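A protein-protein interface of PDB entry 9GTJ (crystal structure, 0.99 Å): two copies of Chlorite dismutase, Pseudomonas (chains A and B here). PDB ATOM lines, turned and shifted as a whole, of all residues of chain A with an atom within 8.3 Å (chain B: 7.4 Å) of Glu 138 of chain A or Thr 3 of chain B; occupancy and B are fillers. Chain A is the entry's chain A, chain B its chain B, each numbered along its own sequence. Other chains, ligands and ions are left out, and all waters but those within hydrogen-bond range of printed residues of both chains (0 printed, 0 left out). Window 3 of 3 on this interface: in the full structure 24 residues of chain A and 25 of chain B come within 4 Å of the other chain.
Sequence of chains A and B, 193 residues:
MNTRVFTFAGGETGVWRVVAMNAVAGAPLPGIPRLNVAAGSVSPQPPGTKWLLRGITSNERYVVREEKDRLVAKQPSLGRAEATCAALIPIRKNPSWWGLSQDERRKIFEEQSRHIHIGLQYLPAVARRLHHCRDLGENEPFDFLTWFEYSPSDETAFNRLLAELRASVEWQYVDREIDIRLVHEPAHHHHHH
Glu 138 of chain A touches just these residues of chain B: Thr 3, Arg 4 and Val 5. Of the printed residues of chain B, Gly 137 of chain A touches Arg 4 (3.7 Å) and Ile 56 (3.9 Å). Printed residues of chain A within 4 Å of Val 5 of chain B: Glu 138 (3.3 Å). Printed residues of chain B within 4 Å of Arg 134 of chain A: Arg 4 (2.9 Å). Of the printed residues of chain B, Asp 135 of chain A touches Arg 4 (2.9 Å) and Ile 56 (3.6 Å). Printed residues of chain A within 4 Å of Arg 4 of chain B: Arg 134, Asp 135, Gly 137 and Glu 138. Ser 41 of chain B touches none of the printed residues of chain A. The nearest printed residue of chain A that does not touch Thr 3 of chain B is Gly 137 of chain A (8.8 Å). The nearest printed residue of chain A that does not touch Arg 4 of chain B is Leu 136 of chain A (6.1 Å).
O of Arg 4 of chain B sits at hydrogen-bond distance from N of Thr 57 of chain B, 2.9 Å away. O of Val 5 of chain B sits at hydrogen-bond distance from N of Gly 40 of chain B.
Of the 11 printed residues of chain A, 4 touch a printed residue of chain B. Of the 11 printed residues of chain B, 4 touch a printed residue of chain A. Hydrophobic or aromatic side chains of chain B within 4 Å of the printed part of chain A: Val 5 and Ile 56. Among the printed residues, Asp or Glu carboxylates within 4 Å of a Lys or Arg side-chain nitrogen of the other chain: Asp 135 of chain A with Arg 4 of chain B (2.9 Å).
NH1 of Arg 4 of chain B lies within hydrogen-bond range of O of Arg 134 of chain A. The side-chain carboxylate of Asp 135 of chain A lies within salt-bridge range of the guanidinium group of Arg 4 of chain B (2.9 Å). The backbone NH (N) of Arg 4 of chain B sits at hydrogen-bond distance from the side-chain carboxylate (OE1) of Glu 138 of chain A (2.9 Å). The backbone NH (N) of Val 5 of chain B is in hydrogen-bond range of the side-chain carboxylate (OE2) of Glu 138 of chain A.
Among the printed residues, pairs that only touch across the chains: Asp 135 of chain A with Ile 56 of chain B (3.6 Å), Gly 137 of chain A with Arg 4 of chain B (3.7 Å), Gly 137 of chain A with Ile 56 of chain B (3.9 Å) and Glu 138 of chain A with Thr 3 of chain B (3.4 Å).
No position is printed for both chains. Of the 8 pairs that touch across the chains among the printed residues, none has its exchanged pair printed and touching as well.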
ATOM      1  N   CYS A 133     -21.663 -16.089 -19.046  1.00  0.00           N
ATOM      2  CA  CYS A 133     -21.056 -16.923 -20.062  1.00  0.00           C
ATOM      3  C   CYS A 133     -20.348 -18.148 -19.508  1.00  0.00           C
ATOM      4  O   CYS A 133     -20.097 -19.092 -20.279  1.00  0.00           O
ATOM      5  CB  CYS A 133     -20.013 -16.176 -20.869  1.00  0.00           C
ATOM      6  SG  CYS A 133     -20.540 -14.568 -21.502  1.00  0.00           S
ATOM      7  N   ARG A 134     -19.946 -18.148 -18.226  1.00  0.00           N
ATOM      8  CA  ARG A 134     -18.957 -19.132 -17.786  1.00  0.00           C
ATOM      9  C   ARG A 134     -19.541 -20.530 -17.630  1.00  0.00           C
ATOM     10  O   ARG A 134     -18.784 -21.497 -17.505  1.00  0.00           O
ATOM     11  CB  ARG A 134     -18.254 -18.640 -16.531  1.00  0.00           C
ATOM     12  CG  ARG A 134     -17.007 -19.358 -16.140  1.00  0.00           C
ATOM     13  CD  ARG A 134     -16.304 -18.689 -14.974  1.00  0.00           C
ATOM     14  NE  ARG A 134     -15.060 -19.323 -14.643  1.00  0.00           N
ATOM     15  CZ  ARG A 134     -14.919 -20.388 -13.887  1.00  0.00           C
ATOM     16  NH1 ARG A 134     -15.971 -20.944 -13.361  1.00  0.00           N
ATOM     17  NH2 ARG A 134     -13.700 -20.877 -13.686  1.00  0.00           N
ATOM     18  N   ASP A 135     -20.862 -20.666 -17.642  1.00  0.00           N
ATOM     19  CA  ASP A 135     -21.457 -21.979 -17.572  1.00  0.00           C
ATOM     20  C   ASP A 135     -21.962 -22.459 -18.928  1.00  0.00           C
ATOM     21  O   ASP A 135     -22.526 -23.528 -19.041  1.00  0.00           O
ATOM     22  CB  ASP A 135     -22.471 -22.030 -16.451  1.00  0.00           C
ATOM     23  CG  ASP A 135     -21.855 -21.711 -15.097  1.00  0.00           C
ATOM     24  OD1 ASP A 135     -20.771 -22.214 -14.784  1.00  0.00           O
ATOM     25  OD2 ASP A 135     -22.500 -20.981 -14.344  1.00  0.00           O
ATOM     26  N   LEU A 136     -21.667 -21.711 -19.994  1.00  0.00           N
ATOM     27  CA  LEU A 136     -21.814 -22.237 -21.354  1.00  0.00           C
ATOM     28  C   LEU A 136     -20.709 -23.271 -21.682  1.00  0.00           C
ATOM     29  O   LEU A 136     -20.881 -24.143 -22.517  1.00  0.00           O
ATOM     30  CB  LEU A 136     -21.780 -21.092 -22.372  1.00  0.00           C
ATOM     31  CG  LEU A 136     -22.743 -19.910 -22.236  1.00  0.00           C
ATOM     32  CD1 LEU A 136     -22.353 -18.809 -23.211  1.00  0.00           C
ATOM     33  CD2 LEU A 136     -24.188 -20.271 -22.458  1.00  0.00           C
ATOM     34  N   GLY A 137     -19.507 -23.120 -21.110  1.00  0.00           N
ATOM     35  CA  GLY A 137     -18.361 -23.963 -21.388  1.00  0.00           C
ATOM     36  C   GLY A 137     -17.111 -23.325 -20.807  1.00  0.00           C
ATOM     37  O   GLY A 137     -17.171 -22.254 -20.219  1.00  0.00           O
ATOM     38  N   GLU A 138     -15.989 -24.009 -21.005  1.00  0.00           N
ATOM     39  CA  GLU A 138     -14.702 -23.668 -20.426  1.00  0.00           C
ATOM     40  C   GLU A 138     -13.957 -22.678 -21.338  1.00  0.00           C
ATOM     41  O   GLU A 138     -12.890 -22.159 -20.957  1.00  0.00           O
ATOM     42  CB  GLU A 138     -13.990 -25.026 -20.163  1.00  0.00           C
ATOM     43  CG  GLU A 138     -14.977 -26.244 -20.075  1.00  0.00           C
ATOM     44  CD  GLU A 138     -14.505 -27.644 -19.661  1.00  0.00           C
ATOM     45  OE1 GLU A 138     -13.557 -27.659 -18.821  1.00  0.00           O
ATOM     46  OE2 GLU A 138     -15.164 -28.759 -20.088  1.00  0.00           O
ATOM     47  N   ASN A 139     -14.503 -22.393 -22.541  1.00  0.00           N
ATOM     48  CA  ASN A 139     -13.759 -21.770 -23.624  1.00  0.00           C
ATOM     49  C   ASN A 139     -14.444 -20.498 -24.116  1.00  0.00           C
ATOM     50  O   ASN A 139     -14.203 -20.093 -25.251  1.00  0.00           O
ATOM     51  CB  ASN A 139     -13.546 -22.768 -24.758  1.00  0.00           C
ATOM     52  CG  ASN A 139     -12.836 -24.021 -24.285  1.00  0.00           C
ATOM     53  OD1 ASN A 139     -11.726 -23.951 -23.753  1.00  0.00           O
ATOM     54  ND2 ASN A 139     -13.474 -25.168 -24.457  1.00  0.00           N
ATOM     55  N   GLU A 140     -15.226 -19.811 -23.262  1.00  0.00           N
ATOM     56  CA  GLU A 140     -15.802 -18.542 -23.676  1.00  0.00           C
ATOM     57  C   GLU A 140     -14.779 -17.453 -23.429  1.00  0.00           C
ATOM     58  O   GLU A 140     -14.073 -17.512 -22.412  1.00  0.00           O
ATOM     59  CB  GLU A 140     -17.090 -18.248 -22.918  1.00  0.00           C
ATOM     60  CG  GLU A 140     -18.091 -19.346 -23.042  1.00  0.00           C
ATOM     61  CD  GLU A 140     -18.578 -19.574 -24.449  1.00  0.00           C
ATOM     62  OE1 GLU A 140     -18.771 -18.587 -25.204  1.00  0.00           O
ATOM     63  OE2 GLU A 140     -18.698 -20.753 -24.797  1.00  0.00           O
ATOM     64  N   PRO A 141     -14.688 -16.433 -24.288  1.00  0.00           N
ATOM     65  CA  PRO A 141     -13.656 -15.430 -24.088  1.00  0.00           C
ATOM     66  C   PRO A 141     -13.879 -14.539 -22.879  1.00  0.00           C
ATOM     67  O   PRO A 141     -12.920 -13.974 -22.365  1.00  0.00           O
ATOM     68  CB  PRO A 141     -13.672 -14.659 -25.405  1.00  0.00           C
ATOM     69  CG  PRO A 141     -15.036 -14.893 -25.977  1.00  0.00           C
ATOM     70  CD  PRO A 141     -15.399 -16.291 -25.569  1.00  0.00           C
ATOM     71  N   PHE A 142     -15.159 -14.323 -22.514  1.00  0.00           N
ATOM     72  CA  PHE A 142     -15.500 -13.493 -21.380  1.00  0.00           C
ATOM     73  C   PHE A 142     -16.363 -14.277 -20.418  1.00  0.00           C
ATOM     74  O   PHE A 142     -16.952 -15.295 -20.792  1.00  0.00           O
ATOM     75  CB  PHE A 142     -16.202 -12.204 -21.830  1.00  0.00           C
ATOM     76  CG  PHE A 142     -15.366 -11.430 -22.824  1.00  0.00           C
ATOM     77  CD1 PHE A 142     -14.373 -10.573 -22.419  1.00  0.00           C
ATOM     78  CD2 PHE A 142     -15.567 -11.650 -24.172  1.00  0.00           C
ATOM     79  CE1 PHE A 142     -13.591  -9.917 -23.371  1.00  0.00           C
ATOM     80  CE2 PHE A 142     -14.785 -11.014 -25.111  1.00  0.00           C
ATOM     81  CZ  PHE A 142     -13.815 -10.151 -24.699  1.00  0.00           C
ATOM     82  N   ASP A 143     -16.461 -13.797 -19.182  1.00  0.00           N
ATOM     83  CA  ASP A 143     -17.374 -14.383 -18.204  1.00  0.00           C
ATOM     84  C   ASP A 143     -18.748 -13.737 -18.186  1.00  0.00           C
ATOM     85  O   ASP A 143     -19.721 -14.403 -17.834  1.00  0.00           O
ATOM     86  CB  ASP A 143     -16.790 -14.304 -16.796  1.00  0.00           C
ATOM     87  CG  ASP A 143     -15.528 -15.132 -16.612  1.00  0.00           C
ATOM     88  OD1 ASP A 143     -15.455 -16.229 -17.224  1.00  0.00           O
ATOM     89  OD2 ASP A 143     -14.632 -14.696 -15.859  1.00  0.00           O
ATOM     90  N   THR B   3     -11.624 -30.656 -16.648  1.00  0.00           N
ATOM     91  CA  THR B   3     -12.883 -30.741 -17.436  1.00  0.00           C
ATOM     92  C   THR B   3     -14.040 -30.358 -16.515  1.00  0.00           C
ATOM     93  O   THR B   3     -14.159 -30.874 -15.413  1.00  0.00           O
ATOM     94  CB  THR B   3     -13.106 -32.196 -17.873  1.00  0.00           C
ATOM     95  OG1 THR B   3     -12.068 -32.454 -18.826  1.00  0.00           O
ATOM     96  CG2 THR B   3     -14.460 -32.461 -18.493  1.00  0.00           C
ATOM     97  N   ARG B   4     -14.917 -29.463 -16.997  1.00  0.00           N
ATOM     98  CA  ARG B   4     -16.108 -29.079 -16.257  1.00  0.00           C
ATOM     99  C   ARG B   4     -17.400 -29.691 -16.801  1.00  0.00           C
ATOM    100  O   ARG B   4     -18.360 -29.833 -16.064  1.00  0.00           O
ATOM    101  CB  ARG B   4     -16.207 -27.559 -16.251  1.00  0.00           C
ATOM    102  CG  ARG B   4     -15.082 -26.874 -15.495  1.00  0.00           C
ATOM    103  CD  ARG B   4     -15.107 -25.369 -15.647  1.00  0.00           C
ATOM    104  NE  ARG B   4     -16.374 -24.829 -15.174  1.00  0.00           N
ATOM    105  CZ  ARG B   4     -17.060 -23.837 -15.719  1.00  0.00           C
ATOM    106  NH1 ARG B   4     -16.552 -23.106 -16.688  1.00  0.00           N
ATOM    107  NH2 ARG B   4     -18.286 -23.604 -15.289  1.00  0.00           N
ATOM    108  N   VAL B   5     -17.451 -29.957 -18.105  1.00  0.00           N
ATOM    109  CA  VAL B   5     -18.657 -30.414 -18.764  1.00  0.00           C
ATOM    110  C   VAL B   5     -18.704 -31.934 -18.768  1.00  0.00           C
ATOM    111  O   VAL B   5     -17.724 -32.578 -19.166  1.00  0.00           O
ATOM    112  CB  VAL B   5     -18.770 -29.878 -20.200  1.00  0.00           C
ATOM    113  CG1 VAL B   5     -19.981 -30.446 -20.939  1.00  0.00           C
ATOM    114  CG2 VAL B   5     -18.826 -28.354 -20.204  1.00  0.00           C
ATOM    115  N   PHE B   6     -19.855 -32.478 -18.370  1.00  0.00           N
ATOM    116  CA  PHE B   6     -20.079 -33.903 -18.396  1.00  0.00           C
ATOM    117  C   PHE B   6     -21.417 -34.187 -19.050  1.00  0.00           C
ATOM    118  O   PHE B   6     -22.389 -33.463 -18.830  1.00  0.00           O
ATOM    119  CB  PHE B   6     -20.007 -34.510 -16.998  1.00  0.00           C
ATOM    120  CG  PHE B   6     -18.623 -34.432 -16.412  1.00  0.00           C
ATOM    121  CD1 PHE B   6     -18.230 -33.284 -15.727  1.00  0.00           C
ATOM    122  CD2 PHE B   6     -17.668 -35.439 -16.619  1.00  0.00           C
ATOM    123  CE1 PHE B   6     -16.953 -33.152 -15.221  1.00  0.00           C
ATOM    124  CE2 PHE B   6     -16.378 -35.299 -16.108  1.00  0.00           C
ATOM    125  CZ  PHE B   6     -16.040 -34.166 -15.399  1.00  0.00           C
ATOM    126  N   ALA B  38     -19.441 -39.112 -20.170  1.00  0.00           N
ATOM    127  CA  ALA B  38     -18.409 -38.595 -21.043  1.00  0.00           C
ATOM    128  C   ALA B  38     -18.003 -37.195 -20.590  1.00  0.00           C
ATOM    129  O   ALA B  38     -18.834 -36.379 -20.270  1.00  0.00           O
ATOM    130  CB  ALA B  38     -18.900 -38.518 -22.471  1.00  0.00           C
ATOM    131  N   ALA B  39     -16.711 -36.878 -20.671  1.00  0.00           N
ATOM    132  CA  ALA B  39     -16.163 -35.579 -20.327  1.00  0.00           C
ATOM    133  C   ALA B  39     -16.034 -34.704 -21.571  1.00  0.00           C
ATOM    134  O   ALA B  39     -15.620 -35.161 -22.629  1.00  0.00           O
ATOM    135  CB  ALA B  39     -14.812 -35.792 -19.685  1.00  0.00           C
ATOM    136  N   GLY B  40     -16.287 -33.402 -21.406  1.00  0.00           N
ATOM    137  CA  GLY B  40     -15.946 -32.367 -22.378  1.00  0.00           C
ATOM    138  C   GLY B  40     -17.134 -31.844 -23.187  1.00  0.00           C
ATOM    139  O   GLY B  40     -18.227 -32.368 -23.148  1.00  0.00           O
ATOM    140  N   SER B  41     -16.891 -30.797 -23.973  1.00  0.00           N
ATOM    141  CA  SER B  41     -17.931 -30.071 -24.673  1.00  0.00           C
ATOM    142  C   SER B  41     -18.273 -30.615 -26.062  1.00  0.00           C
ATOM    143  O   SER B  41     -19.230 -30.125 -26.676  1.00  0.00           O
ATOM    144  CB  SER B  41     -17.449 -28.641 -24.767  1.00  0.00           C
ATOM    145  OG  SER B  41     -16.096 -28.600 -25.243  1.00  0.00           O
ATOM    146  N   ILE B  56     -22.610 -28.872 -16.105  1.00  0.00           N
ATOM    147  CA  ILE B  56     -21.274 -28.312 -15.971  1.00  0.00           C
ATOM    148  C   ILE B  56     -20.996 -28.062 -14.492  1.00  0.00           C
ATOM    149  O   ILE B  56     -21.835 -27.518 -13.770  1.00  0.00           O
ATOM    150  CB  ILE B  56     -21.106 -27.065 -16.859  1.00  0.00           C
ATOM    151  CG1 ILE B  56     -19.637 -26.670 -17.026  1.00  0.00           C
ATOM    152  CG2 ILE B  56     -21.926 -25.875 -16.377  1.00  0.00           C
ATOM    153  CD1 ILE B  56     -19.388 -25.563 -18.009  1.00  0.00           C
ATOM    154  N   THR B  57     -19.800 -28.439 -14.030  1.00  0.00           N
ATOM    155  CA  THR B  57     -19.421 -28.028 -12.687  1.00  0.00           C
ATOM    156  C   THR B  57     -19.168 -26.518 -12.695  1.00  0.00           C
ATOM    157  O   THR B  57     -18.816 -25.955 -13.735  1.00  0.00           O
ATOM    158  CB  THR B  57     -18.215 -28.806 -12.181  1.00  0.00           C
ATOM    159  OG1 THR B  57     -17.082 -28.494 -12.997  1.00  0.00           O
ATOM    160  CG2 THR B  57     -18.442 -30.301 -12.174  1.00  0.00           C
ATOM    161  N   ARG B 129     -20.625 -35.157  -6.879  1.00  0.00           N
ATOM    162  CA  ARG B 129     -20.297 -34.095  -7.818  1.00  0.00           C
ATOM    163  C   ARG B 129     -21.605 -33.421  -8.248  1.00  0.00           C
ATOM    164  O   ARG B 129     -22.594 -34.093  -8.577  1.00  0.00           O
ATOM    165  CB  ARG B 129     -19.526 -34.616  -9.040  1.00  0.00           C
ATOM    166  CG  ARG B 129     -19.075 -33.514  -9.988  1.00  0.00           C
ATOM    167  CD  ARG B 129     -18.165 -34.021 -11.066  1.00  0.00           C
ATOM    168  NE  ARG B 129     -16.868 -34.266 -10.549  1.00  0.00           N
ATOM    169  CZ  ARG B 129     -15.971 -34.959 -11.245  1.00  0.00           C
ATOM    170  NH1 ARG B 129     -16.378 -35.676 -12.274  1.00  0.00           N
ATOM    171  NH2 ARG B 129     -14.708 -35.004 -10.884  1.00  0.00           N
